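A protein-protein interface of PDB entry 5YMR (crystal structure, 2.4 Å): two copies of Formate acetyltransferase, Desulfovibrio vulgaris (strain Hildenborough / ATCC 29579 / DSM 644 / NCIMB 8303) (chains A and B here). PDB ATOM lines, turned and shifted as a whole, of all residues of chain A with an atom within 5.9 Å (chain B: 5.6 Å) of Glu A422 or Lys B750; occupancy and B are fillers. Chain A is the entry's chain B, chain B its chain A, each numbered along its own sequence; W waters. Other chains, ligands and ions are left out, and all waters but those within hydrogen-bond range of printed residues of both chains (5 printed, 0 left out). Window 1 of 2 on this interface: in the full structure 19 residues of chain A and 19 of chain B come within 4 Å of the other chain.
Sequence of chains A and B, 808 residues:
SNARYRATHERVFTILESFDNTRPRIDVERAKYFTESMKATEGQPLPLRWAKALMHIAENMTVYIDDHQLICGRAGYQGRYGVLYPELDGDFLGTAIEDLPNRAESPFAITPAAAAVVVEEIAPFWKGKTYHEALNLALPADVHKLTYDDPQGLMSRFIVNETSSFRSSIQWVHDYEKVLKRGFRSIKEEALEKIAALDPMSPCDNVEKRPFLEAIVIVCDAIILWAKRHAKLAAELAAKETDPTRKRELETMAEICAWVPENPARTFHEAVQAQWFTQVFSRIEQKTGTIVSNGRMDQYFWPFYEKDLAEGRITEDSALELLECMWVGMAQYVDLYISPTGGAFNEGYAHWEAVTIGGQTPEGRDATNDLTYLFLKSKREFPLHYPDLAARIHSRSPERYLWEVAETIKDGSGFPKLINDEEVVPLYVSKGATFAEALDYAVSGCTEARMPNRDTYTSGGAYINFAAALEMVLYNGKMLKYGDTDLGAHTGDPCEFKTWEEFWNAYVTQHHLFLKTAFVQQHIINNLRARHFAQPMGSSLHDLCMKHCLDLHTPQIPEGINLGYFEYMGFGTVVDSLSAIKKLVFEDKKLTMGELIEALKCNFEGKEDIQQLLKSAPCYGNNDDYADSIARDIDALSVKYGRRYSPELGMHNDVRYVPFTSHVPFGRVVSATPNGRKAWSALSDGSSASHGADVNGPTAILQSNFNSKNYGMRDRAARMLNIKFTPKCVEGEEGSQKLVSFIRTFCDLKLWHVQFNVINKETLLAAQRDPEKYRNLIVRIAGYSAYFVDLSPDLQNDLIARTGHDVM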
ATOM      1  N   GLN A 360       9.375 -14.137 -26.152  1.00  0.00           N
ATOM      2  CA  GLN A 360       8.455 -14.994 -26.879  1.00  0.00           C
ATOM      3  C   GLN A 360       8.550 -14.738 -28.380  1.00  0.00           C
ATOM      4  O   GLN A 360       8.931 -13.648 -28.818  1.00  0.00           O
ATOM      5  CB  GLN A 360       7.008 -14.785 -26.378  1.00  0.00           C
ATOM      6  CG  GLN A 360       6.820 -15.186 -24.907  1.00  0.00           C
ATOM      7  CD  GLN A 360       5.448 -14.824 -24.350  1.00  0.00           C
ATOM      8  OE1 GLN A 360       4.440 -15.475 -24.656  1.00  0.00           O
ATOM      9  NE2 GLN A 360       5.411 -13.806 -23.507  1.00  0.00           N
ATOM     10  N   ILE A 393      11.523 -11.196 -20.023  1.00  0.00           N
ATOM     11  CA  ILE A 393      11.002 -12.153 -19.067  1.00  0.00           C
ATOM     12  C   ILE A 393       9.525 -12.386 -19.363  1.00  0.00           C
ATOM     13  O   ILE A 393       8.802 -11.442 -19.707  1.00  0.00           O
ATOM     14  CB  ILE A 393      11.177 -11.644 -17.629  1.00  0.00           C
ATOM     15  CG1 ILE A 393      12.603 -11.158 -17.420  1.00  0.00           C
ATOM     16  CG2 ILE A 393      10.848 -12.757 -16.651  1.00  0.00           C
ATOM     17  CD1 ILE A 393      13.625 -12.226 -17.679  1.00  0.00           C
ATOM     18  N   HIS A 394       9.078 -13.631 -19.203  1.00  0.00           N
ATOM     19  CA  HIS A 394       7.654 -13.968 -19.199  1.00  0.00           C
ATOM     20  C   HIS A 394       7.426 -15.147 -18.251  1.00  0.00           C
ATOM     21  O   HIS A 394       8.364 -15.686 -17.664  1.00  0.00           O
ATOM     22  CB  HIS A 394       7.129 -14.256 -20.614  1.00  0.00           C
ATOM     23  CG  HIS A 394       7.739 -15.458 -21.266  1.00  0.00           C
ATOM     24  ND1 HIS A 394       7.071 -16.654 -21.400  1.00  0.00           N
ATOM     25  CD2 HIS A 394       8.953 -15.640 -21.837  1.00  0.00           C
ATOM     26  CE1 HIS A 394       7.841 -17.520 -22.037  1.00  0.00           C
ATOM     27  NE2 HIS A 394       8.993 -16.931 -22.306  1.00  0.00           N
ATOM     28  N   SER A 395       6.155 -15.496 -18.045  1.00  0.00           N
ATOM     29  CA  SER A 395       5.802 -16.479 -17.027  1.00  0.00           C
ATOM     30  C   SER A 395       6.332 -17.875 -17.328  1.00  0.00           C
ATOM     31  O   SER A 395       6.327 -18.723 -16.430  1.00  0.00           O
ATOM     32  CB  SER A 395       4.296 -16.567 -16.884  1.00  0.00           C
ATOM     33  OG  SER A 395       3.779 -17.174 -18.054  1.00  0.00           O
ATOM     34  N   ARG A 396       6.741 -18.146 -18.570  1.00  0.00           N
ATOM     35  CA  ARG A 396       7.352 -19.420 -18.944  1.00  0.00           C
ATOM     36  C   ARG A 396       8.806 -19.242 -19.404  1.00  0.00           C
ATOM     37  O   ARG A 396       9.327 -20.064 -20.159  1.00  0.00           O
ATOM     38  CB  ARG A 396       6.515 -20.123 -20.024  1.00  0.00           C
ATOM     39  CG  ARG A 396       5.257 -20.871 -19.499  1.00  0.00           C
ATOM     40  CD  ARG A 396       4.126 -20.894 -20.549  1.00  0.00           C
ATOM     41  NE  ARG A 396       3.729 -19.523 -20.860  1.00  0.00           N
ATOM     42  CZ  ARG A 396       4.117 -18.850 -21.937  1.00  0.00           C
ATOM     43  NH1 ARG A 396       4.869 -19.440 -22.863  1.00  0.00           N
ATOM     44  NH2 ARG A 396       3.753 -17.584 -22.090  1.00  0.00           N
ATOM     45  N   ASN A 420       9.502  -7.034 -18.870  1.00  0.00           N
ATOM     46  CA  ASN A 420       8.521  -8.050 -18.519  1.00  0.00           C
ATOM     47  C   ASN A 420       7.446  -8.154 -19.598  1.00  0.00           C
ATOM     48  O   ASN A 420       6.582  -7.284 -19.716  1.00  0.00           O
ATOM     49  CB  ASN A 420       7.918  -7.726 -17.157  1.00  0.00           C
ATOM     50  CG  ASN A 420       6.994  -8.790 -16.670  1.00  0.00           C
ATOM     51  OD1 ASN A 420       6.926  -9.881 -17.241  1.00  0.00           O
ATOM     52  ND2 ASN A 420       6.295  -8.503 -15.578  1.00  0.00           N
ATOM     53  N   ASP A 421       7.473  -9.253 -20.351  1.00  0.00           N
ATOM     54  CA  ASP A 421       6.438  -9.474 -21.353  1.00  0.00           C
ATOM     55  C   ASP A 421       5.043  -9.328 -20.766  1.00  0.00           C
ATOM     56  O   ASP A 421       4.145  -8.778 -21.414  1.00  0.00           O
ATOM     57  CB  ASP A 421       6.598 -10.851 -21.981  1.00  0.00           C
ATOM     58  CG  ASP A 421       7.826 -10.944 -22.841  1.00  0.00           C
ATOM     59  OD1 ASP A 421       8.682 -10.024 -22.804  1.00  0.00           O
ATOM     60  OD2 ASP A 421       7.898 -11.925 -23.595  1.00  0.00           O
ATOM     61  N   GLU A 422       4.834  -9.842 -19.550  1.00  0.00           N
ATOM     62  CA  GLU A 422       3.499  -9.862 -18.966  1.00  0.00           C
ATOM     63  C   GLU A 422       2.969  -8.457 -18.693  1.00  0.00           C
ATOM     64  O   GLU A 422       1.781  -8.296 -18.411  1.00  0.00           O
ATOM     65  CB  GLU A 422       3.493 -10.688 -17.671  1.00  0.00           C
ATOM     66  CG  GLU A 422       3.997 -12.122 -17.789  1.00  0.00           C
ATOM     67  CD  GLU A 422       3.296 -12.902 -18.873  1.00  0.00           C
ATOM     68  OE1 GLU A 422       3.893 -13.855 -19.426  1.00  0.00           O
ATOM     69  OE2 GLU A 422       2.132 -12.569 -19.158  1.00  0.00           O
ATOM     70  N   GLU A 423       3.827  -7.441 -18.699  1.00  0.00           N
ATOM     71  CA  GLU A 423       3.310  -6.083 -18.584  1.00  0.00           C
ATOM     72  C   GLU A 423       3.127  -5.443 -19.954  1.00  0.00           C
ATOM     73  O   GLU A 423       2.124  -4.761 -20.186  1.00  0.00           O
ATOM     74  CB  GLU A 423       4.241  -5.236 -17.709  1.00  0.00           C
ATOM     75  CG  GLU A 423       4.019  -3.718 -17.779  1.00  0.00           C
ATOM     76  CD  GLU A 423       2.869  -3.250 -16.912  1.00  0.00           C
ATOM     77  OE1 GLU A 423       1.889  -4.010 -16.768  1.00  0.00           O
ATOM     78  OE2 GLU A 423       2.948  -2.130 -16.361  1.00  0.00           O
ATOM     79  N   VAL A 424       4.060  -5.682 -20.878  1.00  0.00           N
ATOM     80  CA  VAL A 424       4.030  -5.018 -22.182  1.00  0.00           C
ATOM     81  C   VAL A 424       2.907  -5.571 -23.056  1.00  0.00           C
ATOM     82  O   VAL A 424       2.135  -4.814 -23.652  1.00  0.00           O
ATOM     83  CB  VAL A 424       5.397  -5.148 -22.886  1.00  0.00           C
ATOM     84  CG1 VAL A 424       5.336  -4.581 -24.316  1.00  0.00           C
ATOM     85  CG2 VAL A 424       6.468  -4.467 -22.073  1.00  0.00           C
ATOM     86  N   VAL A 425       2.819  -6.899 -23.188  1.00  0.00           N
ATOM     87  CA  VAL A 425       1.916  -7.479 -24.193  1.00  0.00           C
ATOM     88  C   VAL A 425       0.455  -7.117 -23.922  1.00  0.00           C
ATOM     89  O   VAL A 425      -0.240  -6.701 -24.862  1.00  0.00           O
ATOM     90  CB  VAL A 425       2.172  -8.986 -24.329  1.00  0.00           C
ATOM     91  CG1 VAL A 425       1.082  -9.673 -25.177  1.00  0.00           C
ATOM     92  CG2 VAL A 425       3.551  -9.204 -24.955  1.00  0.00           C
ATOM     93  N   PRO A 426      -0.070  -7.243 -22.701  1.00  0.00           N
ATOM     94  CA  PRO A 426      -1.468  -6.818 -22.499  1.00  0.00           C
ATOM     95  C   PRO A 426      -1.669  -5.341 -22.755  1.00  0.00           C
ATOM     96  O   PRO A 426      -2.646  -4.952 -23.408  1.00  0.00           O
ATOM     97  CB  PRO A 426      -1.756  -7.199 -21.032  1.00  0.00           C
ATOM     98  CG  PRO A 426      -0.790  -8.283 -20.725  1.00  0.00           C
ATOM     99  CD  PRO A 426       0.480  -7.902 -21.501  1.00  0.00           C
ATOM    100  N   CYS A 747       8.121 -10.799 -12.332  1.00  0.00           N
ATOM    101  CA  CYS A 747       7.267 -11.100 -13.477  1.00  0.00           C
ATOM    102  C   CYS A 747       5.798 -11.191 -13.058  1.00  0.00           C
ATOM    103  O   CYS A 747       4.931 -10.558 -13.667  1.00  0.00           O
ATOM    104  CB  CYS A 747       7.733 -12.395 -14.152  1.00  0.00           C
ATOM    105  SG  CYS A 747       6.778 -12.904 -15.597  1.00  0.00           S
ATOM    106  N   LYS A 750       3.627  -8.055 -12.646  1.00  0.00           N
ATOM    107  CA  LYS A 750       3.351  -7.230 -13.813  1.00  0.00           C
ATOM    108  C   LYS A 750       4.138  -5.928 -13.756  1.00  0.00           C
ATOM    109  O   LYS A 750       3.698  -4.898 -14.265  1.00  0.00           O
ATOM    110  CB  LYS A 750       1.851  -6.941 -13.940  1.00  0.00           C
ATOM    111  CG  LYS A 750       0.972  -8.174 -13.730  1.00  0.00           C
ATOM    112  CD  LYS A 750       1.384  -9.310 -14.666  1.00  0.00           C
ATOM    113  CE  LYS A 750       0.641 -10.614 -14.354  1.00  0.00           C
ATOM    114  NZ  LYS A 750      -0.823 -10.503 -14.592  1.00  0.00           N
ATOM    115  N   ASN B 420      -8.857 -19.027 -15.934  1.00  0.00           N
ATOM    116  CA  ASN B 420      -7.532 -18.426 -15.818  1.00  0.00           C
ATOM    117  C   ASN B 420      -7.532 -16.977 -16.297  1.00  0.00           C
ATOM    118  O   ASN B 420      -7.566 -16.715 -17.502  1.00  0.00           O
ATOM    119  CB  ASN B 420      -6.532 -19.247 -16.623  1.00  0.00           C
ATOM    120  CG  ASN B 420      -5.129 -18.705 -16.540  1.00  0.00           C
ATOM    121  OD1 ASN B 420      -4.813 -17.823 -15.727  1.00  0.00           O
ATOM    122  ND2 ASN B 420      -4.263 -19.242 -17.378  1.00  0.00           N
ATOM    123  N   GLU B 422      -5.137 -14.992 -16.690  1.00  0.00           N
ATOM    124  CA  GLU B 422      -4.023 -14.658 -17.571  1.00  0.00           C
ATOM    125  C   GLU B 422      -4.334 -14.969 -19.027  1.00  0.00           C
ATOM    126  O   GLU B 422      -3.684 -14.422 -19.926  1.00  0.00           O
ATOM    127  CB  GLU B 422      -2.781 -15.418 -17.112  1.00  0.00           C
ATOM    128  CG  GLU B 422      -2.436 -15.202 -15.636  1.00  0.00           C
ATOM    129  CD  GLU B 422      -2.269 -13.728 -15.215  1.00  0.00           C
ATOM    130  OE1 GLU B 422      -2.542 -13.409 -14.040  1.00  0.00           O
ATOM    131  OE2 GLU B 422      -1.861 -12.884 -16.034  1.00  0.00           O
ATOM    132  N   GLU B 423      -5.338 -15.803 -19.286  1.00  0.00           N
ATOM    133  CA  GLU B 423      -5.789 -16.011 -20.655  1.00  0.00           C
ATOM    134  C   GLU B 423      -6.961 -15.097 -21.016  1.00  0.00           C
ATOM    135  O   GLU B 423      -6.983 -14.513 -22.108  1.00  0.00           O
ATOM    136  CB  GLU B 423      -6.176 -17.481 -20.854  1.00  0.00           C
ATOM    137  CG  GLU B 423      -7.052 -17.726 -22.078  1.00  0.00           C
ATOM    138  CD  GLU B 423      -6.279 -17.770 -23.388  1.00  0.00           C
ATOM    139  OE1 GLU B 423      -5.245 -17.058 -23.511  1.00  0.00           O
ATOM    140  OE2 GLU B 423      -6.730 -18.511 -24.295  1.00  0.00           O
ATOM    141  N   LYS B 709      -2.662 -24.364 -29.722  1.00  0.00           N
ATOM    142  CA  LYS B 709      -3.242 -23.035 -29.841  1.00  0.00           C
ATOM    143  C   LYS B 709      -2.393 -22.172 -30.779  1.00  0.00           C
ATOM    144  O   LYS B 709      -1.393 -22.613 -31.347  1.00  0.00           O
ATOM    145  CB  LYS B 709      -3.389 -22.406 -28.450  1.00  0.00           C
ATOM    146  CG  LYS B 709      -4.504 -23.095 -27.622  1.00  0.00           C
ATOM    147  CD  LYS B 709      -4.490 -22.732 -26.134  1.00  0.00           C
ATOM    148  CE  LYS B 709      -4.931 -21.300 -25.901  1.00  0.00           C
ATOM    149  NZ  LYS B 709      -4.992 -20.949 -24.452  1.00  0.00           N
ATOM    150  N   TYR B 711      -1.355 -18.422 -30.198  1.00  0.00           N
ATOM    151  CA  TYR B 711      -1.408 -17.240 -29.353  1.00  0.00           C
ATOM    152  C   TYR B 711      -1.135 -15.961 -30.108  1.00  0.00           C
ATOM    153  O   TYR B 711      -1.424 -14.889 -29.568  1.00  0.00           O
ATOM    154  CB  TYR B 711      -0.401 -17.378 -28.192  1.00  0.00           C
ATOM    155  CG  TYR B 711      -0.832 -18.390 -27.165  1.00  0.00           C
ATOM    156  CD1 TYR B 711      -1.679 -18.025 -26.118  1.00  0.00           C
ATOM    157  CD2 TYR B 711      -0.447 -19.740 -27.278  1.00  0.00           C
ATOM    158  CE1 TYR B 711      -2.105 -18.980 -25.164  1.00  0.00           C
ATOM    159  CE2 TYR B 711      -0.852 -20.689 -26.343  1.00  0.00           C
ATOM    160  CZ  TYR B 711      -1.685 -20.307 -25.292  1.00  0.00           C
ATOM    161  OH  TYR B 711      -2.094 -21.252 -24.386  1.00  0.00           O
ATOM    162  N   ARG B 716     -10.159 -16.350 -30.550  1.00  0.00           N
ATOM    163  CA  ARG B 716     -10.199 -17.600 -29.809  1.00  0.00           C
ATOM    164  C   ARG B 716     -11.018 -17.329 -28.557  1.00  0.00           C
ATOM    165  O   ARG B 716     -11.047 -16.197 -28.048  1.00  0.00           O
ATOM    166  CB  ARG B 716      -8.767 -18.097 -29.472  1.00  0.00           C
ATOM    167  CG  ARG B 716      -8.617 -18.948 -28.211  1.00  0.00           C
ATOM    168  CD  ARG B 716      -7.365 -18.599 -27.318  1.00  0.00           C
ATOM    169  NE  ARG B 716      -6.401 -17.817 -28.066  1.00  0.00           N
ATOM    170  CZ  ARG B 716      -5.464 -17.030 -27.550  1.00  0.00           C
ATOM    171  NH1 ARG B 716      -5.307 -16.887 -26.244  1.00  0.00           N
ATOM    172  NH2 ARG B 716      -4.680 -16.384 -28.381  1.00  0.00           N
ATOM    173  N   THR B 745       1.043 -24.354 -13.173  1.00  0.00           N
ATOM    174  CA  THR B 745       1.458 -24.621 -14.541  1.00  0.00           C
ATOM    175  C   THR B 745       0.323 -24.372 -15.527  1.00  0.00           C
ATOM    176  O   THR B 745       0.557 -23.865 -16.629  1.00  0.00           O
ATOM    177  CB  THR B 745       1.976 -26.047 -14.652  1.00  0.00           C
ATOM    178  OG1 THR B 745       3.033 -26.234 -13.702  1.00  0.00           O
ATOM    179  CG2 THR B 745       2.500 -26.291 -16.038  1.00  0.00           C
ATOM    180  N   PHE B 746      -0.903 -24.767 -15.171  1.00  0.00           N
ATOM    181  CA  PHE B 746      -2.063 -24.431 -15.992  1.00  0.00           C
ATOM    182  C   PHE B 746      -2.186 -22.917 -16.204  1.00  0.00           C
ATOM    183  O   PHE B 746      -2.408 -22.459 -17.333  1.00  0.00           O
ATOM    184  CB  PHE B 746      -3.329 -25.028 -15.364  1.00  0.00           C
ATOM    185  CG  PHE B 746      -4.580 -24.245 -15.644  1.00  0.00           C
ATOM    186  CD1 PHE B 746      -5.240 -24.363 -16.852  1.00  0.00           C
ATOM    187  CD2 PHE B 746      -5.083 -23.387 -14.699  1.00  0.00           C
ATOM    188  CE1 PHE B 746      -6.395 -23.627 -17.100  1.00  0.00           C
ATOM    189  CE2 PHE B 746      -6.218 -22.658 -14.935  1.00  0.00           C
ATOM    190  CZ  PHE B 746      -6.883 -22.768 -16.132  1.00  0.00           C
ATOM    191  N   CYS B 747      -2.039 -22.123 -15.131  1.00  0.00           N
ATOM    192  CA  CYS B 747      -2.098 -20.661 -15.258  1.00  0.00           C
ATOM    193  C   CYS B 747      -0.954 -20.129 -16.122  1.00  0.00           C
ATOM    194  O   CYS B 747      -1.173 -19.302 -17.015  1.00  0.00           O
ATOM    195  CB  CYS B 747      -2.085 -20.006 -13.871  1.00  0.00           C
ATOM    196  SG  CYS B 747      -2.089 -18.153 -13.804  1.00  0.00           S
ATOM    197  N   ASP B 748       0.275 -20.584 -15.862  1.00  0.00           N
ATOM    198  CA  ASP B 748       1.439 -20.081 -16.593  1.00  0.00           C
ATOM    199  C   ASP B 748       1.302 -20.300 -18.091  1.00  0.00           C
ATOM    200  O   ASP B 748       1.812 -19.495 -18.887  1.00  0.00           O
ATOM    201  CB  ASP B 748       2.726 -20.783 -16.127  1.00  0.00           C
ATOM    202  CG  ASP B 748       3.174 -20.372 -14.728  1.00  0.00           C
ATOM    203  OD1 ASP B 748       2.674 -19.382 -14.185  1.00  0.00           O
ATOM    204  OD2 ASP B 748       4.039 -21.075 -14.160  1.00  0.00           O
ATOM    205  N   LEU B 749       0.658 -21.398 -18.493  1.00  0.00           N
ATOM    206  CA  LEU B 749       0.504 -21.761 -19.899  1.00  0.00           C
ATOM    207  C   LEU B 749      -0.618 -20.988 -20.582  1.00  0.00           C
ATOM    208  O   LEU B 749      -0.903 -21.251 -21.747  1.00  0.00           O
ATOM    209  CB  LEU B 749       0.265 -23.274 -20.036  1.00  0.00           C
ATOM    210  CG  LEU B 749       1.476 -24.196 -19.737  1.00  0.00           C
ATOM    211  CD1 LEU B 749       1.056 -25.659 -19.556  1.00  0.00           C
ATOM    212  CD2 LEU B 749       2.587 -24.112 -20.796  1.00  0.00           C
ATOM    213  N   LYS B 750      -1.274 -20.064 -19.878  1.00  0.00           N
ATOM    214  CA  LYS B 750      -2.324 -19.230 -20.451  1.00  0.00           C
ATOM    215  C   LYS B 750      -3.474 -20.079 -20.981  1.00  0.00           C
ATOM    216  O   LYS B 750      -4.163 -19.696 -21.924  1.00  0.00           O
ATOM    217  CB  LYS B 750      -1.782 -18.324 -21.560  1.00  0.00           C
ATOM    218  CG  LYS B 750      -0.497 -17.582 -21.186  1.00  0.00           C
ATOM    219  CD  LYS B 750      -0.657 -16.763 -19.927  1.00  0.00           C
ATOM    220  CE  LYS B 750       0.687 -16.144 -19.499  1.00  0.00           C
ATOM    221  NZ  LYS B 750       1.234 -15.146 -20.474  1.00  0.00           N
ATOM    222  N   LEU B 751      -3.712 -21.229 -20.356  1.00  0.00           N
ATOM    223  CA  LEU B 751      -4.872 -22.033 -20.689  1.00  0.00           C
ATOM    224  C   LEU B 751      -6.114 -21.450 -20.025  1.00  0.00           C
ATOM    225  O   LEU B 751      -6.040 -20.827 -18.964  1.00  0.00           O
ATOM    226  CB  LEU B 751      -4.647 -23.477 -20.260  1.00  0.00           C
ATOM    227  CG  LEU B 751      -3.366 -24.033 -20.891  1.00  0.00           C
ATOM    228  CD1 LEU B 751      -3.032 -25.454 -20.429  1.00  0.00           C
ATOM    229  CD2 LEU B 751      -3.541 -24.000 -22.405  1.00  0.00           C
ATOM    230  N   TRP B 752      -7.251 -21.607 -20.693  1.00  0.00           N
ATOM    231  CA  TRP B 752      -8.466 -20.940 -20.236  1.00  0.00           C
ATOM    232  C   TRP B 752      -9.130 -21.668 -19.063  1.00  0.00           C
ATOM    233  O   TRP B 752      -9.586 -21.023 -18.117  1.00  0.00           O
ATOM    234  CB  TRP B 752      -9.443 -20.804 -21.399  1.00  0.00           C
ATOM    235  CG  TRP B 752     -10.650 -19.978 -21.126  1.00  0.00           C
ATOM    236  CD1 TRP B 752     -11.575 -20.167 -20.146  1.00  0.00           C
ATOM    237  CD2 TRP B 752     -11.104 -18.853 -21.898  1.00  0.00           C
ATOM    238  NE1 TRP B 752     -12.558 -19.208 -20.229  1.00  0.00           N
ATOM    239  CE2 TRP B 752     -12.306 -18.403 -21.310  1.00  0.00           C
ATOM    240  CE3 TRP B 752     -10.602 -18.180 -23.029  1.00  0.00           C
ATOM    241  CZ2 TRP B 752     -13.017 -17.308 -21.807  1.00  0.00           C
ATOM    242  CZ3 TRP B 752     -11.305 -17.089 -23.523  1.00  0.00           C
ATOM    243  CH2 TRP B 752     -12.505 -16.664 -22.909  1.00  0.00           C
HETATM  244  O   HOH W   1       2.755 -12.562 -22.181  1.00  0.00           O
HETATM  245  O   HOH W   2       6.096 -18.522 -13.900  1.00  0.00           O
HETATM  246  O   HOH W   3      -1.797 -11.644 -12.291  1.00  0.00           O
HETATM  247  O   HOH W   4       0.869 -13.594 -16.609  1.00  0.00           O
HETATM  248  O   HOH W   5      -0.897 -12.522 -20.095  1.00  0.00           O
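The side-chain hydroxyl (OG) of Ser A395 sits at hydrogen-bond distance from the backbone carbonyl oxygen (O) of Asp B748 (3.2 Å). The guanidinium group of Arg A396 sits at hydrogen-bond distance from the backbone carbonyl oxygen of Asp B748 (2.8 Å). The side-chain carboxylate (OE2) of Glu A422 lies within salt-bridge range of the side-chain amino group (NZ) of Lys B750 (3.0 Å). The side-chain amino group of Lys A750 is in salt-bridge range of the side-chain carboxylate of Glu B422.
The side-chain hydroxyl of Tyr B711 lies within hydrogen-bond range of the backbone carbonyl oxygen of Leu B749 (2.9 Å). The side-chain carboxylate (OE1) of Glu A422 lies within hydrogen-bond range of the backbone NH (N) of Ser A395, at 3.1 Å. NZ of Lys B709 is in hydrogen-bond range of O of Lys B750, at 2.9 Å. OD1 of Asn A420 lies close to N of Glu A422 (3.1 Å). NH2 of Arg A396 is in hydrogen-bond range of OE1 of Gln A360, at 3.4 Å. The side-chain amide oxygen of Asn B420 is in hydrogen-bond range of the backbone NH of Glu B422 (3.0 Å).
Lys B750 touches Ser A395 (CE to OG, 3.6 Å). CD of Arg A396 touches CD2 of Leu B749, at 3.6 Å. NH2 of Arg A396 touches NZ of Lys B750, 3.9 Å away.
Of the printed residues of chain B, Ser A395 touches Asp B748 and Lys B750. Printed residues of chain B within 4 Å of Arg A396: Asp B748 (2.8 Å), Leu B749 (3.6 Å) and Lys B750 (3.9 Å). Glu A422 touches just one residue of chain B: Lys B750. Printed residues of chain A within 4 Å of Glu B422: Lys A750 (3.0 Å). Thr B745 touches none of the printed residues of chain A. Of the printed residues of chain A, Asp B748 touches Ser A395 (3.2 Å) and Arg A396 (2.8 Å). Of the printed residues of chain A, Leu B749 touches Arg A396. Lys B750 touches three residues of chain A. The nearest residue of chain A that does not touch Lys B750 is Gln A360 (5.3 Å).
Glu A422 touches Lys B750, and with the chains exchanged Lys A750 touches Glu B422. Positions printed for both chains: 420, 422, 423, 747 and 750. Of the 7 pairs that touch across the chains among the printed residues, 2 have their exchanged pair printed and touching as well.
Water W2 bridges O of Ser A395 and OD2 of Asp B748. Water W3 bridges the side-chain carboxylate of Glu B422 (2.6 Å) and the side-chain amino group of Lys A750 (2.7 Å). Water W4 lies within hydrogen-bond range of the side-chain carboxylate (OE2) of Glu B422 (2.9 Å) and the side-chain carboxylate (OE2) of Glu A422 (3.0 Å). Water W1 lies within hydrogen-bond range of OE2 of Glu A422 (3.1 Å), NE2 of Gln A360 (3.2 Å) and NZ of Lys B750 (3.5 Å). Water W5 lies within hydrogen-bond range of OE2 of Glu A422 (3.2 Å), O of Glu B422 (3.4 Å) and NZ of Lys B750 (3.4 Å).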
